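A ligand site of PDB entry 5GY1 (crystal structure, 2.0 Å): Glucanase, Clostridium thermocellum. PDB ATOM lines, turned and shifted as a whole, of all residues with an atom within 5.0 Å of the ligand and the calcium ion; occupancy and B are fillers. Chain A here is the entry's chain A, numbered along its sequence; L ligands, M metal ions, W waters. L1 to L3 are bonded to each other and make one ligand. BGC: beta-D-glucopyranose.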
ATOM      1  N   ALA A 143     -14.419   7.273   5.381  1.00  0.00           N
ATOM      2  CA  ALA A 143     -13.602   6.335   4.602  1.00  0.00           C
ATOM      3  C   ALA A 143     -14.420   5.656   3.503  1.00  0.00           C
ATOM      4  O   ALA A 143     -14.051   5.626   2.314  1.00  0.00           O
ATOM      5  CB  ALA A 143     -12.979   5.286   5.537  1.00  0.00           C
ATOM      6  N   GLY A 189     -14.899  -5.765  12.115  1.00  0.00           N
ATOM      7  CA  GLY A 189     -14.437  -7.151  12.191  1.00  0.00           C
ATOM      8  C   GLY A 189     -14.194  -7.802  10.828  1.00  0.00           C
ATOM      9  O   GLY A 189     -13.439  -8.760  10.734  1.00  0.00           O
ATOM     10  N   PHE A 190     -14.864  -7.307   9.781  1.00  0.00           N
ATOM     11  CA  PHE A 190     -14.625  -7.774   8.419  1.00  0.00           C
ATOM     12  C   PHE A 190     -13.788  -6.744   7.663  1.00  0.00           C
ATOM     13  O   PHE A 190     -12.700  -7.066   7.176  1.00  0.00           O
ATOM     14  CB  PHE A 190     -15.949  -8.015   7.688  1.00  0.00           C
ATOM     15  CG  PHE A 190     -16.875  -8.948   8.428  1.00  0.00           C
ATOM     16  CD1 PHE A 190     -16.779 -10.322   8.249  1.00  0.00           C
ATOM     17  CD2 PHE A 190     -17.821  -8.452   9.306  1.00  0.00           C
ATOM     18  CE1 PHE A 190     -17.637 -11.182   8.932  1.00  0.00           C
ATOM     19  CE2 PHE A 190     -18.672  -9.308  10.004  1.00  0.00           C
ATOM     20  CZ  PHE A 190     -18.574 -10.664   9.810  1.00  0.00           C
ATOM     21  N   TYR A 191     -14.303  -5.512   7.613  1.00  0.00           N
ATOM     22  CA  TYR A 191     -13.637  -4.381   6.975  1.00  0.00           C
ATOM     23  C   TYR A 191     -13.707  -3.132   7.873  1.00  0.00           C
ATOM     24  O   TYR A 191     -14.151  -2.068   7.431  1.00  0.00           O
ATOM     25  CB  TYR A 191     -14.222  -4.114   5.579  1.00  0.00           C
ATOM     26  CG  TYR A 191     -13.929  -5.247   4.598  1.00  0.00           C
ATOM     27  CD1 TYR A 191     -12.683  -5.352   3.985  1.00  0.00           C
ATOM     28  CD2 TYR A 191     -14.884  -6.219   4.308  1.00  0.00           C
ATOM     29  CE1 TYR A 191     -12.386  -6.394   3.098  1.00  0.00           C
ATOM     30  CE2 TYR A 191     -14.586  -7.283   3.423  1.00  0.00           C
ATOM     31  CZ  TYR A 191     -13.352  -7.348   2.815  1.00  0.00           C
ATOM     32  OH  TYR A 191     -13.025  -8.370   1.941  1.00  0.00           O
ATOM     33  N   SER A 192     -13.244  -3.269   9.120  1.00  0.00           N
ATOM     34  CA  SER A 192     -13.120  -2.114  10.017  1.00  0.00           C
ATOM     35  C   SER A 192     -12.185  -1.073   9.411  1.00  0.00           C
ATOM     36  O   SER A 192     -11.240  -1.413   8.731  1.00  0.00           O
ATOM     37  CB  SER A 192     -12.515  -2.541  11.358  1.00  0.00           C
ATOM     38  OG  SER A 192     -13.446  -3.356  12.049  1.00  0.00           O
ATOM     39  N   SER A 193     -12.437   0.199   9.700  1.00  0.00           N
ATOM     40  CA  SER A 193     -11.530   1.230   9.218  1.00  0.00           C
ATOM     41  C   SER A 193     -10.350   1.229  10.188  1.00  0.00           C
ATOM     42  O   SER A 193     -10.507   1.603  11.346  1.00  0.00           O
ATOM     43  CB  SER A 193     -12.245   2.580   9.211  1.00  0.00           C
ATOM     44  OG  SER A 193     -11.378   3.614   8.791  1.00  0.00           O
ATOM     45  N   HIS A 194      -9.185   0.789   9.738  1.00  0.00           N
ATOM     46  CA  HIS A 194      -8.021   0.671  10.622  1.00  0.00           C
ATOM     47  C   HIS A 194      -7.183   1.958  10.580  1.00  0.00           C
ATOM     48  O   HIS A 194      -6.827   2.526  11.598  1.00  0.00           O
ATOM     49  CB  HIS A 194      -7.187  -0.556  10.226  1.00  0.00           C
ATOM     50  CG  HIS A 194      -7.903  -1.857  10.401  1.00  0.00           C
ATOM     51  ND1 HIS A 194      -7.777  -2.645  11.530  1.00  0.00           N
ATOM     52  CD2 HIS A 194      -8.762  -2.513   9.580  1.00  0.00           C
ATOM     53  CE1 HIS A 194      -8.531  -3.723  11.399  1.00  0.00           C
ATOM     54  NE2 HIS A 194      -9.136  -3.670  10.227  1.00  0.00           N
ATOM     55  N   SER A 195      -6.918   2.441   9.365  1.00  0.00           N
ATOM     56  CA  SER A 195      -6.086   3.616   9.175  1.00  0.00           C
ATOM     57  C   SER A 195      -6.790   4.955   9.429  1.00  0.00           C
ATOM     58  O   SER A 195      -6.124   5.983   9.482  1.00  0.00           O
ATOM     59  CB  SER A 195      -5.500   3.603   7.751  1.00  0.00           C
ATOM     60  OG  SER A 195      -6.536   3.420   6.778  1.00  0.00           O
ATOM     61  N   GLY A 196      -8.114   4.963   9.561  1.00  0.00           N
ATOM     62  CA  GLY A 196      -8.852   6.225   9.579  1.00  0.00           C
ATOM     63  C   GLY A 196      -9.213   6.657   8.166  1.00  0.00           C
ATOM     64  O   GLY A 196      -9.028   5.915   7.194  1.00  0.00           O
ATOM     65  N   PHE A 197      -9.727   7.888   8.038  1.00  0.00           N
ATOM     66  CA  PHE A 197     -10.345   8.321   6.785  1.00  0.00           C
ATOM     67  C   PHE A 197      -9.533   9.344   5.990  1.00  0.00           C
ATOM     68  O   PHE A 197      -9.905   9.678   4.862  1.00  0.00           O
ATOM     69  CB  PHE A 197     -11.739   8.893   7.061  1.00  0.00           C
ATOM     70  CG  PHE A 197     -11.711  10.073   7.988  1.00  0.00           C
ATOM     71  CD1 PHE A 197     -11.325  11.326   7.526  1.00  0.00           C
ATOM     72  CD2 PHE A 197     -11.990   9.911   9.338  1.00  0.00           C
ATOM     73  CE1 PHE A 197     -11.248  12.422   8.402  1.00  0.00           C
ATOM     74  CE2 PHE A 197     -11.924  10.994  10.217  1.00  0.00           C
ATOM     75  CZ  PHE A 197     -11.556  12.255   9.735  1.00  0.00           C
ATOM     76  N   ASP A 199      -6.702   9.119   4.521  1.00  0.00           N
ATOM     77  CA  ASP A 199      -6.202   8.591   3.247  1.00  0.00           C
ATOM     78  C   ASP A 199      -7.284   8.504   2.166  1.00  0.00           C
ATOM     79  O   ASP A 199      -6.991   8.735   0.991  1.00  0.00           O
ATOM     80  CB  ASP A 199      -5.503   7.243   3.428  1.00  0.00           C
ATOM     81  CG  ASP A 199      -6.376   6.255   4.153  1.00  0.00           C
ATOM     82  OD1 ASP A 199      -6.560   6.405   5.376  1.00  0.00           O
ATOM     83  OD2 ASP A 199      -6.923   5.346   3.499  1.00  0.00           O
ATOM     84  N   GLU A 200      -8.507   8.160   2.535  1.00  0.00           N
ATOM     85  CA  GLU A 200      -9.593   8.132   1.545  1.00  0.00           C
ATOM     86  C   GLU A 200      -9.931   9.533   1.043  1.00  0.00           C
ATOM     87  O   GLU A 200     -10.264   9.694  -0.131  1.00  0.00           O
ATOM     88  CB  GLU A 200     -10.875   7.457   2.071  1.00  0.00           C
ATOM     89  CG  GLU A 200     -10.798   5.935   2.166  1.00  0.00           C
ATOM     90  CD  GLU A 200     -10.145   5.443   3.463  1.00  0.00           C
ATOM     91  OE1 GLU A 200      -9.773   6.290   4.286  1.00  0.00           O
ATOM     92  OE2 GLU A 200      -9.979   4.221   3.688  1.00  0.00           O
ATOM     93  N   ASN A 229      -1.205   8.969   8.765  1.00  0.00           N
ATOM     94  CA  ASN A 229      -0.500   8.326   9.863  1.00  0.00           C
ATOM     95  C   ASN A 229       0.994   8.329   9.606  1.00  0.00           C
ATOM     96  O   ASN A 229       1.409   8.288   8.452  1.00  0.00           O
ATOM     97  CB  ASN A 229      -1.004   6.893  10.055  1.00  0.00           C
ATOM     98  CG  ASN A 229      -2.494   6.857  10.287  1.00  0.00           C
ATOM     99  OD1 ASN A 229      -2.999   7.623  11.092  1.00  0.00           O
ATOM    100  ND2 ASN A 229      -3.210   6.030   9.535  1.00  0.00           N
ATOM    101  N   GLU A 238       3.630   7.063   7.027  1.00  0.00           N
ATOM    102  CA  GLU A 238       3.657   5.595   6.984  1.00  0.00           C
ATOM    103  C   GLU A 238       3.875   5.040   5.570  1.00  0.00           C
ATOM    104  O   GLU A 238       3.151   5.380   4.625  1.00  0.00           O
ATOM    105  CB  GLU A 238       2.355   5.040   7.558  1.00  0.00           C
ATOM    106  CG  GLU A 238       2.285   3.525   7.557  1.00  0.00           C
ATOM    107  CD  GLU A 238       1.289   3.040   8.590  1.00  0.00           C
ATOM    108  OE1 GLU A 238       0.083   2.938   8.275  1.00  0.00           O
ATOM    109  OE2 GLU A 238       1.715   2.838   9.749  1.00  0.00           O
ATOM    110  N   TRP A 241       3.491  -0.697   4.462  1.00  0.00           N
ATOM    111  CA  TRP A 241       2.256  -1.449   4.271  1.00  0.00           C
ATOM    112  C   TRP A 241       1.983  -1.421   2.774  1.00  0.00           C
ATOM    113  O   TRP A 241       2.810  -0.925   1.996  1.00  0.00           O
ATOM    114  CB  TRP A 241       1.103  -0.863   5.103  1.00  0.00           C
ATOM    115  CG  TRP A 241      -0.005  -1.877   5.300  1.00  0.00           C
ATOM    116  CD1 TRP A 241      -1.229  -1.890   4.692  1.00  0.00           C
ATOM    117  CD2 TRP A 241       0.041  -3.052   6.120  1.00  0.00           C
ATOM    118  NE1 TRP A 241      -1.961  -2.983   5.096  1.00  0.00           N
ATOM    119  CE2 TRP A 241      -1.203  -3.716   5.976  1.00  0.00           C
ATOM    120  CE3 TRP A 241       1.001  -3.602   6.988  1.00  0.00           C
ATOM    121  CZ2 TRP A 241      -1.500  -4.902   6.655  1.00  0.00           C
ATOM    122  CZ3 TRP A 241       0.705  -4.784   7.657  1.00  0.00           C
ATOM    123  CH2 TRP A 241      -0.536  -5.418   7.493  1.00  0.00           C
ATOM    124  N   CYS A 244      -4.240  -0.748  -0.385  1.00  0.00           N
ATOM    125  CA  CYS A 244      -5.272  -1.750  -0.149  1.00  0.00           C
ATOM    126  C   CYS A 244      -6.613  -1.117   0.172  1.00  0.00           C
ATOM    127  O   CYS A 244      -6.722   0.107   0.318  1.00  0.00           O
ATOM    128  CB  CYS A 244      -4.865  -2.669   1.007  1.00  0.00           C
ATOM    129  SG  CYS A 244      -4.792  -1.823   2.609  1.00  0.00           S
ATOM    130  N   TRP A 245      -7.617  -1.970   0.342  1.00  0.00           N
ATOM    131  CA  TRP A 245      -8.989  -1.510   0.552  1.00  0.00           C
ATOM    132  C   TRP A 245      -9.127  -0.521   1.724  1.00  0.00           C
ATOM    133  O   TRP A 245     -10.037   0.303   1.716  1.00  0.00           O
ATOM    134  CB  TRP A 245      -9.927  -2.718   0.778  1.00  0.00           C
ATOM    135  CG  TRP A 245      -9.542  -3.548   2.003  1.00  0.00           C
ATOM    136  CD1 TRP A 245      -8.811  -4.696   2.022  1.00  0.00           C
ATOM    137  CD2 TRP A 245      -9.900  -3.274   3.364  1.00  0.00           C
ATOM    138  NE1 TRP A 245      -8.674  -5.163   3.322  1.00  0.00           N
ATOM    139  CE2 TRP A 245      -9.337  -4.305   4.166  1.00  0.00           C
ATOM    140  CE3 TRP A 245     -10.654  -2.269   3.994  1.00  0.00           C
ATOM    141  CZ2 TRP A 245      -9.492  -4.352   5.550  1.00  0.00           C
ATOM    142  CZ3 TRP A 245     -10.799  -2.316   5.379  1.00  0.00           C
ATOM    143  CH2 TRP A 245     -10.230  -3.349   6.137  1.00  0.00           C
ATOM    144  N   ASP A 246      -8.240  -0.625   2.706  1.00  0.00           N
ATOM    145  CA  ASP A 246      -8.280   0.214   3.915  1.00  0.00           C
ATOM    146  C   ASP A 246      -7.481   1.509   3.794  1.00  0.00           C
ATOM    147  O   ASP A 246      -7.725   2.465   4.531  1.00  0.00           O
ATOM    148  CB  ASP A 246      -7.752  -0.567   5.127  1.00  0.00           C
ATOM    149  CG  ASP A 246      -7.885   0.228   6.425  1.00  0.00           C
ATOM    150  OD1 ASP A 246      -9.039   0.477   6.816  1.00  0.00           O
ATOM    151  OD2 ASP A 246      -6.868   0.607   7.029  1.00  0.00           O
ATOM    152  N   ASP A 247      -6.551   1.542   2.844  1.00  0.00           N
ATOM    153  CA  ASP A 247      -5.535   2.595   2.848  1.00  0.00           C
ATOM    154  C   ASP A 247      -4.926   2.755   1.457  1.00  0.00           C
ATOM    155  O   ASP A 247      -4.165   1.916   0.976  1.00  0.00           O
ATOM    156  CB  ASP A 247      -4.473   2.281   3.897  1.00  0.00           C
ATOM    157  CG  ASP A 247      -3.549   3.454   4.169  1.00  0.00           C
ATOM    158  OD1 ASP A 247      -3.608   4.479   3.448  1.00  0.00           O
ATOM    159  OD2 ASP A 247      -2.748   3.347   5.116  1.00  0.00           O
ATOM    160  N   TYR A 250      -0.819   5.345  -0.489  1.00  0.00           N
ATOM    161  CA  TYR A 250       0.319   4.912  -1.302  1.00  0.00           C
ATOM    162  C   TYR A 250       0.090   5.252  -2.781  1.00  0.00           C
ATOM    163  O   TYR A 250       0.919   5.938  -3.389  1.00  0.00           O
ATOM    164  CB  TYR A 250       0.583   3.416  -1.104  1.00  0.00           C
ATOM    165  CG  TYR A 250       0.642   3.044   0.369  1.00  0.00           C
ATOM    166  CD1 TYR A 250       1.814   3.182   1.111  1.00  0.00           C
ATOM    167  CD2 TYR A 250      -0.504   2.621   1.044  1.00  0.00           C
ATOM    168  CE1 TYR A 250       1.848   2.857   2.469  1.00  0.00           C
ATOM    169  CE2 TYR A 250      -0.478   2.291   2.388  1.00  0.00           C
ATOM    170  CZ  TYR A 250       0.701   2.425   3.086  1.00  0.00           C
ATOM    171  OH  TYR A 250       0.726   2.122   4.441  1.00  0.00           O
ATOM    172  N   ASP A 297       1.282 -10.184   5.163  1.00  0.00           N
ATOM    173  CA  ASP A 297       0.453 -10.618   6.285  1.00  0.00           C
ATOM    174  C   ASP A 297      -0.116 -11.990   5.956  1.00  0.00           C
ATOM    175  O   ASP A 297      -0.100 -12.431   4.804  1.00  0.00           O
ATOM    176  CB  ASP A 297      -0.696  -9.627   6.512  1.00  0.00           C
ATOM    177  CG  ASP A 297      -1.443  -9.869   7.816  1.00  0.00           C
ATOM    178  OD1 ASP A 297      -0.806 -10.136   8.857  1.00  0.00           O
ATOM    179  OD2 ASP A 297      -2.694  -9.791   7.791  1.00  0.00           O
ATOM    180  N   TRP A 299      -3.272 -12.809   5.835  1.00  0.00           N
ATOM    181  CA  TRP A 299      -4.448 -12.708   4.963  1.00  0.00           C
ATOM    182  C   TRP A 299      -4.057 -12.199   3.581  1.00  0.00           C
ATOM    183  O   TRP A 299      -3.402 -11.148   3.499  1.00  0.00           O
ATOM    184  CB  TRP A 299      -5.425 -11.668   5.521  1.00  0.00           C
ATOM    185  CG  TRP A 299      -6.138 -12.107   6.756  1.00  0.00           C
ATOM    186  CD1 TRP A 299      -5.891 -11.715   8.046  1.00  0.00           C
ATOM    187  CD2 TRP A 299      -7.245 -13.014   6.802  1.00  0.00           C
ATOM    188  NE1 TRP A 299      -6.766 -12.341   8.893  1.00  0.00           N
ATOM    189  CE2 TRP A 299      -7.617 -13.131   8.158  1.00  0.00           C
ATOM    190  CE3 TRP A 299      -7.950 -13.738   5.832  1.00  0.00           C
ATOM    191  CZ2 TRP A 299      -8.669 -13.960   8.575  1.00  0.00           C
ATOM    192  CZ3 TRP A 299      -8.991 -14.554   6.244  1.00  0.00           C
ATOM    193  CH2 TRP A 299      -9.344 -14.661   7.607  1.00  0.00           C
ATOM    194  N   ARG A 303      -2.790 -10.863  -2.875  1.00  0.00           N
ATOM    195  CA  ARG A 303      -3.504  -9.602  -3.085  1.00  0.00           C
ATOM    196  C   ARG A 303      -2.607  -8.387  -2.841  1.00  0.00           C
ATOM    197  O   ARG A 303      -2.494  -7.485  -3.679  1.00  0.00           O
ATOM    198  CB  ARG A 303      -4.752  -9.576  -2.177  1.00  0.00           C
ATOM    199  CG  ARG A 303      -5.397  -8.204  -1.911  1.00  0.00           C
ATOM    200  CD  ARG A 303      -4.946  -7.575  -0.579  1.00  0.00           C
ATOM    201  NE  ARG A 303      -4.933  -8.501   0.574  1.00  0.00           N
ATOM    202  CZ  ARG A 303      -5.897  -8.594   1.482  1.00  0.00           C
ATOM    203  NH1 ARG A 303      -7.029  -7.908   1.350  1.00  0.00           N
ATOM    204  NH2 ARG A 303      -5.767  -9.410   2.523  1.00  0.00           N
ATOM    205  N   TYR A 304      -1.894  -8.388  -1.720  1.00  0.00           N
ATOM    206  CA  TYR A 304      -1.056  -7.249  -1.408  1.00  0.00           C
ATOM    207  C   TYR A 304       0.109  -7.110  -2.389  1.00  0.00           C
ATOM    208  O   TYR A 304       0.413  -6.012  -2.830  1.00  0.00           O
ATOM    209  CB  TYR A 304      -0.507  -7.353   0.008  1.00  0.00           C
ATOM    210  CG  TYR A 304      -1.524  -7.188   1.119  1.00  0.00           C
ATOM    211  CD1 TYR A 304      -2.340  -6.066   1.197  1.00  0.00           C
ATOM    212  CD2 TYR A 304      -1.620  -8.146   2.121  1.00  0.00           C
ATOM    213  CE1 TYR A 304      -3.257  -5.913   2.251  1.00  0.00           C
ATOM    214  CE2 TYR A 304      -2.480  -7.986   3.196  1.00  0.00           C
ATOM    215  CZ  TYR A 304      -3.311  -6.875   3.246  1.00  0.00           C
ATOM    216  OH  TYR A 304      -4.179  -6.766   4.310  1.00  0.00           O
ATOM    217  N   TYR A 414      -8.790  -8.800  -3.990  1.00  0.00           N
ATOM    218  CA  TYR A 414      -7.676  -9.641  -4.400  1.00  0.00           C
ATOM    219  C   TYR A 414      -7.384  -9.494  -5.897  1.00  0.00           C
ATOM    220  O   TYR A 414      -6.229  -9.454  -6.329  1.00  0.00           O
ATOM    221  CB  TYR A 414      -8.005 -11.124  -4.160  1.00  0.00           C
ATOM    222  CG  TYR A 414      -8.041 -11.597  -2.722  1.00  0.00           C
ATOM    223  CD1 TYR A 414      -8.179 -10.688  -1.672  1.00  0.00           C
ATOM    224  CD2 TYR A 414      -7.934 -12.949  -2.430  1.00  0.00           C
ATOM    225  CE1 TYR A 414      -8.186 -11.137  -0.363  1.00  0.00           C
ATOM    226  CE2 TYR A 414      -7.951 -13.421  -1.121  1.00  0.00           C
ATOM    227  CZ  TYR A 414      -8.085 -12.500  -0.098  1.00  0.00           C
ATOM    228  OH  TYR A 414      -8.113 -12.918   1.211  1.00  0.00           O
HETATM  229  C2  BGC L   1      -9.065  -8.960   4.800  1.00  0.00           C
HETATM  230  C3  BGC L   1      -7.818  -8.374   5.471  1.00  0.00           C
HETATM  231  C4  BGC L   1      -8.156  -7.891   6.880  1.00  0.00           C
HETATM  232  C5  BGC L   1      -8.924  -8.929   7.719  1.00  0.00           C
HETATM  233  C6  BGC L   1      -9.572  -8.301   8.960  1.00  0.00           C
HETATM  234  C1  BGC L   1      -9.678 -10.052   5.693  1.00  0.00           C
HETATM  235  O1  BGC L   1     -10.903 -10.555   5.138  1.00  0.00           O
HETATM  236  O2  BGC L   1      -8.668  -9.536   3.546  1.00  0.00           O
HETATM  237  O3  BGC L   1      -7.275  -7.326   4.648  1.00  0.00           O
HETATM  238  O4  BGC L   1      -6.960  -7.550   7.582  1.00  0.00           O
HETATM  239  O5  BGC L   1      -9.994  -9.445   6.939  1.00  0.00           O
HETATM  240  O6  BGC L   1     -10.272  -7.095   8.597  1.00  0.00           O
HETATM  241  C2  BGC L   2      -5.741  -6.093   8.972  1.00  0.00           C
HETATM  242  C3  BGC L   2      -5.447  -4.628   9.236  1.00  0.00           C
HETATM  243  C4  BGC L   2      -5.066  -3.874   7.968  1.00  0.00           C
HETATM  244  C5  BGC L   2      -6.161  -4.084   6.920  1.00  0.00           C
HETATM  245  C6  BGC L   2      -5.752  -3.547   5.552  1.00  0.00           C
HETATM  246  C1  BGC L   2      -6.847  -6.161   7.918  1.00  0.00           C
HETATM  247  O2  BGC L   2      -6.281  -6.582  10.200  1.00  0.00           O
HETATM  248  O3  BGC L   2      -4.468  -4.469  10.256  1.00  0.00           O
HETATM  249  O4  BGC L   2      -4.979  -2.505   8.347  1.00  0.00           O
HETATM  250  O5  BGC L   2      -6.430  -5.477   6.746  1.00  0.00           O
HETATM  251  O6  BGC L   2      -4.502  -4.105   5.085  1.00  0.00           O
HETATM  252  C2  BGC L   3      -3.740  -0.443   7.849  1.00  0.00           C
HETATM  253  C3  BGC L   3      -2.344   0.181   7.855  1.00  0.00           C
HETATM  254  C4  BGC L   3      -1.526  -0.267   9.053  1.00  0.00           C
HETATM  255  C5  BGC L   3      -1.577  -1.791   9.128  1.00  0.00           C
HETATM  256  C6  BGC L   3      -0.717  -2.342  10.266  1.00  0.00           C
HETATM  257  C1  BGC L   3      -3.683  -1.957   8.076  1.00  0.00           C
HETATM  258  O2  BGC L   3      -4.368  -0.145   6.603  1.00  0.00           O
HETATM  259  O3  BGC L   3      -2.486   1.602   7.862  1.00  0.00           O
HETATM  260  O4  BGC L   3      -0.186   0.204   8.843  1.00  0.00           O
HETATM  261  O5  BGC L   3      -2.935  -2.219   9.256  1.00  0.00           O
HETATM  262  O6  BGC L   3      -1.438  -2.226  11.496  1.00  0.00           O
HETATM  263 CA    CA M   1      -8.329   4.499   5.481  1.00  0.00          CA
HETATM  264  O   HOH W   1     -10.470  -9.079   1.344  1.00  0.00           O
HETATM  265  O   HOH W   2     -12.942  -9.457   5.964  1.00  0.00           O
HETATM  266  O   HOH W   3     -11.543  -5.466  10.397  1.00  0.00           O
HETATM  267  O   HOH W   4      -4.389  -8.340   6.272  1.00  0.00           O
HETATM  268  O   HOH W   5      -3.006   2.688  10.370  1.00  0.00           O
HETATM  269  O   HOH W   6      -1.852   4.734   7.188  1.00  0.00           O
HETATM  270  O   HOH W   7      -9.712   2.993   6.755  1.00  0.00           O
HETATM  271  O   HOH W   8     -10.155 -11.490   2.441  1.00  0.00           O
HETATM  272  O   HOH W   9      -4.185  -9.073  10.069  1.00  0.00           O
HETATM  273  O   HOH W  10     -11.995 -12.534   3.618  1.00  0.00           O
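SG of Cys 244 lies within hydrogen-bond range of O6 of BGC L2 (3.4 Å). The side-chain hydroxyl (OH) of Tyr 304 is in hydrogen-bond range of an oxygen (O6) of BGC L2. The guanidinium group (NH2) of Arg 303 lies within hydrogen-bond range of an oxygen (O2) of BGC L1 (3.1 Å). OE1 of Glu 238 sits at hydrogen-bond distance from O4 of BGC L3 (2.8 Å). O3 of BGC L1 lies within hydrogen-bond range of NE1 of Trp 245 (2.9 Å). O of Phe 190 lies within hydrogen-bond range of O6 of BGC L1, 2.8 Å away. NE1 of Trp 241 is in hydrogen-bond range of O6 of BGC L2 (2.8 Å). O2 of BGC L3 lies within hydrogen-bond range of OD2 of Asp 246 (2.6 Å). The side-chain carboxylate (OD2) of Asp 247 is in hydrogen-bond range of an oxygen (O3) of BGC L3 (3.3 Å).
O of Ser 195 sits at hydrogen-bond distance from ND2 of Asn 229, at 2.9 Å. The backbone NH (N) of Glu 238 is in hydrogen-bond range of the backbone carbonyl oxygen (O) of Asn 229 (2.9 Å). The side-chain carboxylate (OD1) of Asp 246 lies within hydrogen-bond range of the backbone NH (N) of His 194 (2.9 Å). N of Asp 246 sits close to SG of Cys 244 (3.7 Å). O of Ser 192 sits close to NE2 of His 194 (3.4 Å). NH2 of Arg 303 lies within hydrogen-bond range of O of Trp 299 (3.1 Å).
Merely in contact with the ligand: His 194 and Trp 299. 12 residues have an atom within 4 Å of the ligand: Phe 190, His 194, Ser 195, Glu 238, Trp 241, Cys 244, Trp 245, Asp 246, Asp 247, Trp 299, Arg 303 and Tyr 304.
The nearest printed residue that does not touch the calcium ion is Asp 247 (4.3 Å).
The calcium ion is bound by O of Asp 246 (2.3 Å), O of Gly 196 (2.3 Å), water W7 (2.4 Å), OE2 of Glu 200 (2.5 Å), OG of Ser 195 (2.5 Å), OD2 of Asp 199 (2.6 Å), OE1 of Glu 200 (2.6 Å) and OD1 of Asp 199 (2.6 Å).
Water W7 lies within hydrogen-bond range of OD1 of Asp 246 (2.6 Å) and OG of Ser 193 (2.7 Å). Water W8 lies within hydrogen-bond range of O2 of BGC L1 (2.7 Å) and OH of Tyr 414 (2.8 Å). Water W1 lies within hydrogen-bond range of the side-chain hydroxyl of Tyr 191 and an oxygen (O2) of BGC L1. Water W4 lies within hydrogen-bond range of OH of Tyr 304 (2.5 Å), OD2 of Asp 297 (2.7 Å) and O4 of BGC L1 (3.0 Å). Water W9 lies within hydrogen-bond range of the side-chain carboxylate of Asp 297 and an oxygen (O2) of BGC L2. Water W6 lies within hydrogen-bond range of OD2 of Asp 247, OE1 of Glu 238, ND2 of Asn 229 and O3 of BGC L3.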
